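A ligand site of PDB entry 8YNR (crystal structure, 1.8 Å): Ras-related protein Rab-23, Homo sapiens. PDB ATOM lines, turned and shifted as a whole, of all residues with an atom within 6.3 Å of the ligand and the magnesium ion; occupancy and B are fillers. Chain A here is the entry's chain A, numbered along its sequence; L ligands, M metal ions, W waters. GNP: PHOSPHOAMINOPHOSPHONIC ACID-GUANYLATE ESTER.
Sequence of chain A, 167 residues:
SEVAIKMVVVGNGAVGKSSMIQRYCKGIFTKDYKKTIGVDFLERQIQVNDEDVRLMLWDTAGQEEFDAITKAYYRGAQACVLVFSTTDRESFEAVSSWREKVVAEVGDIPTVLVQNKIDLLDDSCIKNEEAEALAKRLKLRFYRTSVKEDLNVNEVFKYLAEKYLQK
Of the 32 residues printed, 2 come within 4 Å of the magnesium ion.
The nearest printed residue that does not touch the magnesium ion is Asp 59 (4.1 Å).
The magnesium ion is bound by an oxygen (O2G) of the ligand (2.0 Å), an oxygen (O1B) of the ligand (2.1 Å), the side-chain hydroxyl of Thr 36 (2.1 Å), water W5 (2.1 Å), water W4 (2.1 Å) and the side-chain hydroxyl of Ser 18 (2.1 Å).
The magnesium ion has six donor atoms within binding distance.
The backbone carbonyl oxygen (O) of Val 15 lies within hydrogen-bond range of the side-chain amide nitrogen (ND2) of Asn 116 (2.9 Å).
The side-chain hydroxyl (OG) of Ser 18 sits close to the side-chain carboxylate (OD2) of Asp 59, at 2.5 Å.
N of Glu 149 lies within hydrogen-bond range of OG of Ser 146 (3.1 Å).
NZ of Lys 17 is in hydrogen-bond range of O of Asn 12 (2.9 Å).
NZ of Lys 17 is in hydrogen-bond range of O of Gly 11 (3.1 Å).
The backbone NH (N) of Val 147 lies within hydrogen-bond range of the side-chain amide oxygen (OD1) of Asn 116.
O of Thr 145 lies within hydrogen-bond range of N of Lys 117, at 3.1 Å.
O of Ala 14 is in hydrogen-bond range of NZ of Lys 117, at 2.8 Å.
N of Ala 14 lies close to N3B of the ligand, 3.0 Å away.
O of Asn 12 touches O2B of the ligand, 3.99 Å away.
CA of Gly 13 touches O3G of the ligand, 3.4 Å away.
Phe 29 touches the ligand.
Lys 35 touches the ligand.
C of Ala 61 touches O3G of the ligand, at 3.6 Å.
Leu 120 touches the ligand (CD1 to N2, 3.5 Å).
Ser 146 touches the ligand.
Within 4 Å of the ligand: Asn 12, Gly 13, Ala 14, Val 15, Gly 16, Lys 17, Ser 18, Ser 19, Phe 29, Thr 30, Lys 31, Tyr 33, Lys 35, Thr 36, Ala 61, Gly 62, Asn 116, Lys 117, Asp 119, Leu 120, Ser 146, Val 147 and Lys 148.
Along chain A the residues within 4 Å of the ligand span positions 12 to 148.
Water W5 bridges the side-chain carboxylate of Asp 59 (2.6 Å) and the backbone carbonyl oxygen of Thr 60 (2.8 Å).
Water W4 lies within hydrogen-bond range of an oxygen (O1A) of the ligand (2.6 Å) and the backbone carbonyl oxygen (O) of Lys 34 (2.8 Å).
Water W2 lies within hydrogen-bond range of O of Asp 32, O1A of the ligand and N of Lys 34.
Water W1 lies within hydrogen-bond range of NZ of Lys 117 (3.0 Å) and N3 of the ligand (3.1 Å).
Water W6 bridges the backbone carbonyl oxygen (O) of Lys 31 (3.1 Å) and an oxygen (O2') of the ligand (3.1 Å).
An oxygen (O2A) of the ligand sits at hydrogen-bond distance from the backbone NH (N) of Ser 19, at 2.8 Å.
N of Val 15 sits at hydrogen-bond distance from O2B of the ligand (3.4 Å).
O3' of the ligand is in hydrogen-bond range of O of Lys 31.
N of Gly 16 lies within hydrogen-bond range of O2B of the ligand (3.0 Å).
O3G of the ligand is in hydrogen-bond range of N of Gly 62, at 2.6 Å.
An oxygen (O2A) of the ligand lies within hydrogen-bond range of the side-chain hydroxyl (OG) of Ser 19, 2.7 Å away.
An oxygen (O2A) of the ligand sits at hydrogen-bond distance from the backbone NH (N) of Ser 18 (3.5 Å).
N of Thr 36 lies close to O2G of the ligand (3.3 Å).
The side-chain hydroxyl of Tyr 33 sits at hydrogen-bond distance from an oxygen (O1G) of the ligand (2.7 Å).
The backbone NH (N) of Lys 17 sits at hydrogen-bond distance from an oxygen (O2B) of the ligand (2.9 Å).
The backbone carbonyl oxygen (O) of Thr 30 is in hydrogen-bond range of an oxygen (O2') of the ligand, 2.7 Å away.
The backbone NH (N) of Lys 148 sits at hydrogen-bond distance from an oxygen (O6) of the ligand.
A nitrogen (N7) of the ligand is in hydrogen-bond range of the side-chain amide nitrogen (ND2) of Asn 116, at 3.1 Å.
The backbone NH (N) of Val 147 lies within hydrogen-bond range of an oxygen (O6) of the ligand (2.9 Å).
A nitrogen (N1) of the ligand sits at hydrogen-bond distance from the side-chain carboxylate (OD1) of Asp 119, 3.0 Å away.
The side-chain amino group (NZ) of Lys 17 is in salt-bridge range of an oxygen (O2B) of the ligand (2.7 Å).
O4' of the ligand is in hydrogen-bond range of NZ of Lys 117, at 3.2 Å.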
ATOM      1  N   GLY A  11      -6.106 -35.671  -1.772  1.00  0.00           N
ATOM      2  CA  GLY A  11      -7.214 -34.736  -1.699  1.00  0.00           C
ATOM      3  C   GLY A  11      -7.080 -33.712  -2.805  1.00  0.00           C
ATOM      4  O   GLY A  11      -6.055 -33.603  -3.466  1.00  0.00           O
ATOM      5  N   ASN A  12      -8.136 -32.915  -2.964  1.00  0.00           N
ATOM      6  CA  ASN A  12      -8.176 -31.960  -4.069  1.00  0.00           C
ATOM      7  C   ASN A  12      -7.038 -30.924  -4.005  1.00  0.00           C
ATOM      8  O   ASN A  12      -6.412 -30.708  -2.973  1.00  0.00           O
ATOM      9  CB  ASN A  12      -9.515 -31.244  -4.089  1.00  0.00           C
ATOM     10  CG  ASN A  12     -10.592 -32.050  -4.770  1.00  0.00           C
ATOM     11  OD1 ASN A  12     -10.437 -33.251  -4.991  1.00  0.00           O
ATOM     12  ND2 ASN A  12     -11.690 -31.385  -5.132  1.00  0.00           N
ATOM     13  N   GLY A  13      -6.807 -30.260  -5.144  1.00  0.00           N
ATOM     14  CA  GLY A  13      -5.796 -29.209  -5.165  1.00  0.00           C
ATOM     15  C   GLY A  13      -6.113 -28.113  -4.166  1.00  0.00           C
ATOM     16  O   GLY A  13      -7.267 -27.735  -3.982  1.00  0.00           O
ATOM     17  N   ALA A  14      -5.070 -27.618  -3.499  1.00  0.00           N
ATOM     18  CA  ALA A  14      -5.090 -26.473  -2.583  1.00  0.00           C
ATOM     19  C   ALA A  14      -5.693 -26.773  -1.223  1.00  0.00           C
ATOM     20  O   ALA A  14      -5.828 -25.853  -0.440  1.00  0.00           O
ATOM     21  CB  ALA A  14      -5.803 -25.247  -3.198  1.00  0.00           C
ATOM     22  N   VAL A  15      -5.999 -28.036  -0.871  1.00  0.00           N
ATOM     23  CA  VAL A  15      -6.537 -28.303   0.466  1.00  0.00           C
ATOM     24  C   VAL A  15      -5.458 -28.144   1.529  1.00  0.00           C
ATOM     25  O   VAL A  15      -5.780 -28.002   2.714  1.00  0.00           O
ATOM     26  CB  VAL A  15      -7.189 -29.694   0.579  1.00  0.00           C
ATOM     27  CG1 VAL A  15      -8.375 -29.821  -0.318  1.00  0.00           C
ATOM     28  CG2 VAL A  15      -6.187 -30.806   0.293  1.00  0.00           C
ATOM     29  N   GLY A  16      -4.189 -28.207   1.153  1.00  0.00           N
ATOM     30  CA  GLY A  16      -3.121 -28.003   2.109  1.00  0.00           C
ATOM     31  C   GLY A  16      -2.247 -29.220   2.373  1.00  0.00           C
ATOM     32  O   GLY A  16      -1.626 -29.320   3.426  1.00  0.00           O
ATOM     33  N   LYS A  17      -2.178 -30.156   1.393  1.00  0.00           N
ATOM     34  CA  LYS A  17      -1.409 -31.392   1.558  1.00  0.00           C
ATOM     35  C   LYS A  17       0.072 -31.106   1.712  1.00  0.00           C
ATOM     36  O   LYS A  17       0.718 -31.610   2.638  1.00  0.00           O
ATOM     37  CB  LYS A  17      -1.644 -32.335   0.355  1.00  0.00           C
ATOM     38  CG  LYS A  17      -3.111 -32.769   0.171  1.00  0.00           C
ATOM     39  CD  LYS A  17      -3.326 -33.619  -1.078  1.00  0.00           C
ATOM     40  CE  LYS A  17      -2.841 -32.931  -2.351  1.00  0.00           C
ATOM     41  NZ  LYS A  17      -3.735 -31.718  -2.679  1.00  0.00           N
ATOM     42  N   SER A  18       0.653 -30.350   0.772  1.00  0.00           N
ATOM     43  CA  SER A  18       2.065 -29.999   0.897  1.00  0.00           C
ATOM     44  C   SER A  18       2.325 -29.235   2.186  1.00  0.00           C
ATOM     45  O   SER A  18       3.357 -29.416   2.827  1.00  0.00           O
ATOM     46  CB  SER A  18       2.531 -29.131  -0.281  1.00  0.00           C
ATOM     47  OG  SER A  18       2.415 -29.792  -1.527  1.00  0.00           O
ATOM     48  N   SER A  19       1.432 -28.283   2.516  1.00  0.00           N
ATOM     49  CA  SER A  19       1.654 -27.511   3.724  1.00  0.00           C
ATOM     50  C   SER A  19       1.655 -28.407   4.951  1.00  0.00           C
ATOM     51  O   SER A  19       2.430 -28.200   5.893  1.00  0.00           O
ATOM     52  CB  SER A  19       0.591 -26.414   3.843  1.00  0.00           C
ATOM     53  OG  SER A  19       0.682 -25.545   2.742  1.00  0.00           O
ATOM     54  N   MET A  20       0.761 -29.399   4.968  1.00  0.00           N
ATOM     55  CA  MET A  20       0.655 -30.278   6.137  1.00  0.00           C
ATOM     56  C   MET A  20       1.936 -31.082   6.300  1.00  0.00           C
ATOM     57  O   MET A  20       2.448 -31.247   7.426  1.00  0.00           O
ATOM     58  CB  MET A  20      -0.564 -31.192   5.972  1.00  0.00           C
ATOM     59  CG  MET A  20      -0.803 -32.242   7.082  1.00  0.00           C
ATOM     60  SD  MET A  20      -2.374 -33.099   6.808  1.00  0.00           S
ATOM     61  CE  MET A  20      -3.523 -31.704   6.805  1.00  0.00           C
ATOM     62  N   PHE A  29       5.445 -22.970   8.045  1.00  0.00           N
ATOM     63  CA  PHE A  29       4.181 -22.813   7.352  1.00  0.00           C
ATOM     64  C   PHE A  29       4.452 -22.163   6.006  1.00  0.00           C
ATOM     65  O   PHE A  29       4.988 -21.049   5.947  1.00  0.00           O
ATOM     66  CB  PHE A  29       3.158 -22.013   8.127  1.00  0.00           C
ATOM     67  CG  PHE A  29       1.887 -21.835   7.374  1.00  0.00           C
ATOM     68  CD1 PHE A  29       1.261 -22.939   6.831  1.00  0.00           C
ATOM     69  CD2 PHE A  29       1.366 -20.591   7.149  1.00  0.00           C
ATOM     70  CE1 PHE A  29       0.097 -22.791   6.125  1.00  0.00           C
ATOM     71  CE2 PHE A  29       0.207 -20.446   6.435  1.00  0.00           C
ATOM     72  CZ  PHE A  29      -0.409 -21.542   5.911  1.00  0.00           C
ATOM     73  N   THR A  30       4.117 -22.881   4.940  1.00  0.00           N
ATOM     74  CA  THR A  30       4.283 -22.391   3.580  1.00  0.00           C
ATOM     75  C   THR A  30       3.039 -21.583   3.203  1.00  0.00           C
ATOM     76  O   THR A  30       1.957 -22.144   3.004  1.00  0.00           O
ATOM     77  CB  THR A  30       4.550 -23.555   2.623  1.00  0.00           C
ATOM     78  OG1 THR A  30       3.535 -24.557   2.756  1.00  0.00           O
ATOM     79  CG2 THR A  30       5.883 -24.214   2.929  1.00  0.00           C
ATOM     80  N   LYS A  31       3.189 -20.259   3.151  1.00  0.00           N
ATOM     81  CA  LYS A  31       2.069 -19.362   2.820  1.00  0.00           C
ATOM     82  C   LYS A  31       1.785 -19.250   1.317  1.00  0.00           C
ATOM     83  O   LYS A  31       0.638 -18.999   0.928  1.00  0.00           O
ATOM     84  CB  LYS A  31       2.359 -17.989   3.392  1.00  0.00           C
ATOM     85  CG  LYS A  31       3.199 -18.019   4.665  1.00  0.00           C
ATOM     86  CD  LYS A  31       3.888 -16.683   4.896  1.00  0.00           C
ATOM     87  CE  LYS A  31       5.198 -16.884   5.659  1.00  0.00           C
ATOM     88  NZ  LYS A  31       6.008 -15.625   5.769  1.00  0.00           N
ATOM     89  N   ASP A  32       2.787 -19.406   0.462  1.00  0.00           N
ATOM     90  CA  ASP A  32       2.574 -19.293  -0.976  1.00  0.00           C
ATOM     91  C   ASP A  32       1.977 -20.589  -1.528  1.00  0.00           C
ATOM     92  O   ASP A  32       2.334 -21.683  -1.080  1.00  0.00           O
ATOM     93  CB  ASP A  32       3.904 -19.006  -1.694  1.00  0.00           C
ATOM     94  CG  ASP A  32       4.511 -17.677  -1.295  1.00  0.00           C
ATOM     95  OD1 ASP A  32       3.775 -16.800  -0.794  1.00  0.00           O
ATOM     96  OD2 ASP A  32       5.728 -17.495  -1.502  1.00  0.00           O
ATOM     97  N   TYR A  33       1.095 -20.483  -2.509  1.00  0.00           N
ATOM     98  CA  TYR A  33       0.543 -21.676  -3.152  1.00  0.00           C
ATOM     99  C   TYR A  33       1.220 -21.875  -4.504  1.00  0.00           C
ATOM    100  O   TYR A  33       1.141 -21.002  -5.365  1.00  0.00           O
ATOM    101  CB  TYR A  33      -0.965 -21.583  -3.315  1.00  0.00           C
ATOM    102  CG  TYR A  33      -1.585 -22.739  -4.068  1.00  0.00           C
ATOM    103  CD1 TYR A  33      -1.046 -24.031  -3.958  1.00  0.00           C
ATOM    104  CD2 TYR A  33      -2.684 -22.551  -4.900  1.00  0.00           C
ATOM    105  CE1 TYR A  33      -1.582 -25.087  -4.648  1.00  0.00           C
ATOM    106  CE2 TYR A  33      -3.246 -23.633  -5.591  1.00  0.00           C
ATOM    107  CZ  TYR A  33      -2.675 -24.898  -5.450  1.00  0.00           C
ATOM    108  OH  TYR A  33      -3.189 -25.986  -6.117  1.00  0.00           O
ATOM    109  N   LYS A  34       1.901 -23.006  -4.669  1.00  0.00           N
ATOM    110  CA  LYS A  34       2.356 -23.495  -5.951  1.00  0.00           C
ATOM    111  C   LYS A  34       1.910 -24.944  -6.064  1.00  0.00           C
ATOM    112  O   LYS A  34       2.120 -25.714  -5.118  1.00  0.00           O
ATOM    113  CB  LYS A  34       3.876 -23.403  -6.090  1.00  0.00           C
ATOM    114  CG  LYS A  34       4.411 -21.974  -6.046  1.00  0.00           C
ATOM    115  CD  LYS A  34       5.926 -21.946  -6.275  1.00  0.00           C
ATOM    116  CE  LYS A  34       6.507 -20.614  -5.857  1.00  0.00           C
ATOM    117  NZ  LYS A  34       7.917 -20.405  -6.283  1.00  0.00           N
ATOM    118  N   LYS A  35       1.290 -25.313  -7.168  1.00  0.00           N
ATOM    119  CA  LYS A  35       0.924 -26.715  -7.335  1.00  0.00           C
ATOM    120  C   LYS A  35       2.191 -27.568  -7.335  1.00  0.00           C
ATOM    121  O   LYS A  35       3.178 -27.232  -7.976  1.00  0.00           O
ATOM    122  CB  LYS A  35       0.143 -26.921  -8.635  1.00  0.00           C
ATOM    123  CG  LYS A  35      -1.283 -26.459  -8.546  1.00  0.00           C
ATOM    124  CD  LYS A  35      -1.907 -26.176  -9.897  1.00  0.00           C
ATOM    125  CE  LYS A  35      -3.321 -25.625  -9.743  1.00  0.00           C
ATOM    126  NZ  LYS A  35      -3.937 -25.239 -11.050  1.00  0.00           N
ATOM    127  N   THR A  36       2.149 -28.665  -6.599  1.00  0.00           N
ATOM    128  CA  THR A  36       3.299 -29.532  -6.467  1.00  0.00           C
ATOM    129  C   THR A  36       3.677 -30.122  -7.820  1.00  0.00           C
ATOM    130  O   THR A  36       2.809 -30.505  -8.612  1.00  0.00           O
ATOM    131  CB  THR A  36       2.980 -30.615  -5.446  1.00  0.00           C
ATOM    132  OG1 THR A  36       2.707 -29.995  -4.175  1.00  0.00           O
ATOM    133  CG2 THR A  36       4.151 -31.598  -5.259  1.00  0.00           C
ATOM    134  N   ASP A  59       4.456 -36.593  -1.291  1.00  0.00           N
ATOM    135  CA  ASP A  59       3.643 -35.427  -1.637  1.00  0.00           C
ATOM    136  C   ASP A  59       3.574 -35.330  -3.154  1.00  0.00           C
ATOM    137  O   ASP A  59       4.613 -35.404  -3.825  1.00  0.00           O
ATOM    138  CB  ASP A  59       4.265 -34.167  -1.046  1.00  0.00           C
ATOM    139  CG  ASP A  59       3.369 -32.947  -1.200  1.00  0.00           C
ATOM    140  OD1 ASP A  59       2.149 -33.136  -1.196  1.00  0.00           O
ATOM    141  OD2 ASP A  59       3.911 -31.828  -1.369  1.00  0.00           O
ATOM    142  N   THR A  60       2.362 -35.175  -3.695  1.00  0.00           N
ATOM    143  CA  THR A  60       2.207 -34.877  -5.121  1.00  0.00           C
ATOM    144  C   THR A  60       0.969 -33.992  -5.283  1.00  0.00           C
ATOM    145  O   THR A  60       0.146 -33.851  -4.368  1.00  0.00           O
ATOM    146  CB  THR A  60       2.127 -36.156  -5.977  1.00  0.00           C
ATOM    147  OG1 THR A  60       2.365 -35.855  -7.354  1.00  0.00           O
ATOM    148  CG2 THR A  60       0.765 -36.850  -5.820  1.00  0.00           C
ATOM    149  N   ALA A  61       0.806 -33.410  -6.479  1.00  0.00           N
ATOM    150  CA  ALA A  61      -0.332 -32.514  -6.685  1.00  0.00           C
ATOM    151  C   ALA A  61      -1.639 -33.288  -6.720  1.00  0.00           C
ATOM    152  O   ALA A  61      -1.738 -34.386  -7.267  1.00  0.00           O
ATOM    153  CB  ALA A  61      -0.165 -31.712  -7.980  1.00  0.00           C
ATOM    154  N   GLY A  62      -2.688 -32.697  -6.129  1.00  0.00           N
ATOM    155  CA  GLY A  62      -4.000 -33.309  -6.156  1.00  0.00           C
ATOM    156  C   GLY A  62      -4.644 -33.261  -7.530  1.00  0.00           C
ATOM    157  O   GLY A  62      -4.827 -34.313  -8.149  1.00  0.00           O
ATOM    158  N   ASN A 116      -8.916 -29.693   6.937  1.00  0.00           N
ATOM    159  CA  ASN A 116      -7.856 -28.729   7.162  1.00  0.00           C
ATOM    160  C   ASN A 116      -8.409 -27.294   7.008  1.00  0.00           C
ATOM    161  O   ASN A 116      -9.528 -27.081   6.561  1.00  0.00           O
ATOM    162  CB  ASN A 116      -6.702 -28.978   6.188  1.00  0.00           C
ATOM    163  CG  ASN A 116      -5.496 -28.106   6.455  1.00  0.00           C
ATOM    164  OD1 ASN A 116      -5.166 -27.859   7.615  1.00  0.00           O
ATOM    165  ND2 ASN A 116      -4.824 -27.619   5.380  1.00  0.00           N
ATOM    166  N   LYS A 117      -7.579 -26.322   7.391  1.00  0.00           N
ATOM    167  CA  LYS A 117      -7.883 -24.893   7.321  1.00  0.00           C
ATOM    168  C   LYS A 117      -8.982 -24.519   8.293  1.00  0.00           C
ATOM    169  O   LYS A 117      -9.729 -23.562   8.084  1.00  0.00           O
ATOM    170  CB  LYS A 117      -8.255 -24.425   5.897  1.00  0.00           C
ATOM    171  CG  LYS A 117      -7.232 -24.816   4.821  1.00  0.00           C
ATOM    172  CD  LYS A 117      -7.428 -23.994   3.532  1.00  0.00           C
ATOM    173  CE  LYS A 117      -6.641 -24.628   2.328  1.00  0.00           C
ATOM    174  NZ  LYS A 117      -6.655 -23.705   1.123  1.00  0.00           N
ATOM    175  N   ILE A 118      -9.074 -25.253   9.412  1.00  0.00           N
ATOM    176  CA  ILE A 118     -10.154 -25.004  10.352  1.00  0.00           C
ATOM    177  C   ILE A 118     -10.086 -23.580  10.926  1.00  0.00           C
ATOM    178  O   ILE A 118     -11.099 -23.076  11.437  1.00  0.00           O
ATOM    179  CB  ILE A 118     -10.155 -26.097  11.447  1.00  0.00           C
ATOM    180  CG1 ILE A 118     -11.517 -26.163  12.139  1.00  0.00           C
ATOM    181  CG2 ILE A 118      -9.024 -25.883  12.435  1.00  0.00           C
ATOM    182  CD1 ILE A 118     -12.591 -26.850  11.306  1.00  0.00           C
ATOM    183  N   ASP A 119      -8.935 -22.912  10.821  1.00  0.00           N
ATOM    184  CA  ASP A 119      -8.827 -21.513  11.214  1.00  0.00           C
ATOM    185  C   ASP A 119      -9.703 -20.585  10.372  1.00  0.00           C
ATOM    186  O   ASP A 119     -10.018 -19.462  10.809  1.00  0.00           O
ATOM    187  CB  ASP A 119      -7.387 -21.025  11.137  1.00  0.00           C
ATOM    188  CG  ASP A 119      -6.780 -21.209   9.769  1.00  0.00           C
ATOM    189  OD1 ASP A 119      -6.534 -22.372   9.404  1.00  0.00           O
ATOM    190  OD2 ASP A 119      -6.566 -20.191   9.065  1.00  0.00           O
ATOM    191  N   LEU A 120     -10.131 -21.018   9.184  1.00  0.00           N
ATOM    192  CA  LEU A 120     -11.022 -20.192   8.367  1.00  0.00           C
ATOM    193  C   LEU A 120     -12.490 -20.525   8.589  1.00  0.00           C
ATOM    194  O   LEU A 120     -13.305 -20.362   7.682  1.00  0.00           O
ATOM    195  CB  LEU A 120     -10.674 -20.378   6.896  1.00  0.00           C
ATOM    196  CG  LEU A 120      -9.171 -20.290   6.631  1.00  0.00           C
ATOM    197  CD1 LEU A 120      -8.910 -20.710   5.202  1.00  0.00           C
ATOM    198  CD2 LEU A 120      -8.740 -18.846   6.886  1.00  0.00           C
ATOM    199  N   THR A 145      -7.968 -29.898  11.433  1.00  0.00           N
ATOM    200  CA  THR A 145      -6.637 -29.386  11.625  1.00  0.00           C
ATOM    201  C   THR A 145      -6.531 -27.968  11.101  1.00  0.00           C
ATOM    202  O   THR A 145      -7.328 -27.533  10.257  1.00  0.00           O
ATOM    203  CB  THR A 145      -5.593 -30.240  10.928  1.00  0.00           C
ATOM    204  OG1 THR A 145      -5.646 -30.045   9.501  1.00  0.00           O
ATOM    205  CG2 THR A 145      -5.841 -31.714  11.297  1.00  0.00           C
ATOM    206  N   SER A 146      -5.532 -27.262  11.595  1.00  0.00           N
ATOM    207  CA  SER A 146      -5.045 -26.031  10.980  1.00  0.00           C
ATOM    208  C   SER A 146      -3.529 -26.168  10.829  1.00  0.00           C
ATOM    209  O   SER A 146      -2.794 -26.059  11.815  1.00  0.00           O
ATOM    210  CB  SER A 146      -5.420 -24.786  11.787  1.00  0.00           C
ATOM    211  OG  SER A 146      -4.921 -23.635  11.124  1.00  0.00           O
ATOM    212  N   VAL A 147      -3.079 -26.404   9.598  1.00  0.00           N
ATOM    213  CA  VAL A 147      -1.639 -26.362   9.322  1.00  0.00           C
ATOM    214  C   VAL A 147      -1.101 -24.991   9.687  1.00  0.00           C
ATOM    215  O   VAL A 147      -0.018 -24.869  10.281  1.00  0.00           O
ATOM    216  CB  VAL A 147      -1.346 -26.737   7.856  1.00  0.00           C
ATOM    217  CG1 VAL A 147       0.145 -26.683   7.591  1.00  0.00           C
ATOM    218  CG2 VAL A 147      -1.881 -28.109   7.545  1.00  0.00           C
ATOM    219  N   LYS A 148      -1.873 -23.943   9.386  1.00  0.00           N
ATOM    220  CA  LYS A 148      -1.417 -22.587   9.654  1.00  0.00           C
ATOM    221  C   LYS A 148      -1.128 -22.383  11.136  1.00  0.00           C
ATOM    222  O   LYS A 148      -0.109 -21.782  11.506  1.00  0.00           O
ATOM    223  CB  LYS A 148      -2.458 -21.588   9.179  1.00  0.00           C
ATOM    224  CG  LYS A 148      -2.058 -20.168   9.379  1.00  0.00           C
ATOM    225  CD  LYS A 148      -3.107 -19.211   8.883  1.00  0.00           C
ATOM    226  CE  LYS A 148      -2.702 -17.771   9.259  1.00  0.00           C
ATOM    227  NZ  LYS A 148      -3.755 -16.752   9.061  1.00  0.00           N
ATOM    228  N   GLU A 149      -1.998 -22.887  12.006  1.00  0.00           N
ATOM    229  CA  GLU A 149      -1.876 -22.694  13.442  1.00  0.00           C
ATOM    230  C   GLU A 149      -1.236 -23.888  14.148  1.00  0.00           C
ATOM    231  O   GLU A 149      -1.187 -23.907  15.379  1.00  0.00           O
ATOM    232  CB  GLU A 149      -3.256 -22.380  14.032  1.00  0.00           C
ATOM    233  CG  GLU A 149      -3.895 -21.117  13.399  1.00  0.00           C
ATOM    234  CD  GLU A 149      -3.070 -19.866  13.661  1.00  0.00           C
ATOM    235  OE1 GLU A 149      -2.318 -19.848  14.656  1.00  0.00           O
ATOM    236  OE2 GLU A 149      -3.173 -18.886  12.871  1.00  0.00           O
HETATM  237  PG  GNP L   1      -1.735 -29.173  -4.767  1.00  0.00           P
HETATM  238  O1G GNP L   1      -1.942 -28.342  -5.965  1.00  0.00           O
HETATM  239  O2G GNP L   1      -0.289 -29.406  -4.579  1.00  0.00           O
HETATM  240  O3G GNP L   1      -2.571 -30.382  -4.845  1.00  0.00           O
HETATM  241  N3B GNP L   1      -2.151 -28.312  -3.418  1.00  0.00           N
HETATM  242  PB  GNP L   1      -1.882 -28.668  -1.843  1.00  0.00           P
HETATM  243  O1B GNP L   1      -0.526 -29.230  -1.669  1.00  0.00           O
HETATM  244  O2B GNP L   1      -2.999 -29.465  -1.328  1.00  0.00           O
HETATM  245  O3A GNP L   1      -2.058 -27.248  -1.082  1.00  0.00           O
HETATM  246  PA  GNP L   1      -0.893 -26.378  -0.440  1.00  0.00           P
HETATM  247  O1A GNP L   1      -0.058 -25.957  -1.593  1.00  0.00           O
HETATM  248  O2A GNP L   1      -0.235 -27.004   0.714  1.00  0.00           O
HETATM  249  O5' GNP L   1      -1.790 -25.203   0.188  1.00  0.00           O
HETATM  250  C5' GNP L   1      -2.563 -24.381  -0.692  1.00  0.00           C
HETATM  251  C4' GNP L   1      -2.737 -23.069   0.033  1.00  0.00           C
HETATM  252  O4' GNP L   1      -3.466 -23.298   1.257  1.00  0.00           O
HETATM  253  C3' GNP L   1      -1.452 -22.336   0.416  1.00  0.00           C
HETATM  254  O3' GNP L   1      -1.643 -20.936   0.247  1.00  0.00           O
HETATM  255  C2' GNP L   1      -1.320 -22.624   1.911  1.00  0.00           C
HETATM  256  O2' GNP L   1      -0.668 -21.605   2.658  1.00  0.00           O
HETATM  257  C1' GNP L   1      -2.785 -22.657   2.317  1.00  0.00           C
HETATM  258  N9  GNP L   1      -3.009 -23.435   3.551  1.00  0.00           N
HETATM  259  C8  GNP L   1      -2.579 -24.708   3.855  1.00  0.00           C
HETATM  260  N7  GNP L   1      -2.989 -25.115   5.041  1.00  0.00           N
HETATM  261  C5  GNP L   1      -3.721 -24.056   5.540  1.00  0.00           C
HETATM  262  C6  GNP L   1      -4.383 -23.886   6.770  1.00  0.00           C
HETATM  263  O6  GNP L   1      -4.464 -24.715   7.679  1.00  0.00           O
HETATM  264  N1  GNP L   1      -4.976 -22.632   6.882  1.00  0.00           N
HETATM  265  C2  GNP L   1      -4.945 -21.656   5.927  1.00  0.00           C
HETATM  266  N2  GNP L   1      -5.554 -20.493   6.213  1.00  0.00           N
HETATM  267  N3  GNP L   1      -4.332 -21.802   4.757  1.00  0.00           N
HETATM  268  C4  GNP L   1      -3.746 -23.010   4.628  1.00  0.00           C
HETATM  269 MG    MG M   1       0.967 -29.610  -3.071  1.00  0.00          MG
HETATM  270  O   HOH W   1      -5.960 -21.030   2.230  1.00  0.00           O
HETATM  271  O   HOH W   2       2.391 -24.459  -1.683  1.00  0.00           O
HETATM  272  O   HOH W   3      -5.522 -18.208   4.594  1.00  0.00           O
HETATM  273  O   HOH W   4       1.347 -27.523  -3.159  1.00  0.00           O
HETATM  274  O   HOH W   5       0.662 -31.663  -2.772  1.00  0.00           O
HETATM  275  O   HOH W   6      -1.371 -18.594   3.209  1.00  0.00           O
HETATM  276  O   HOH W   7      -3.283 -29.538  -7.939  1.00  0.00           O
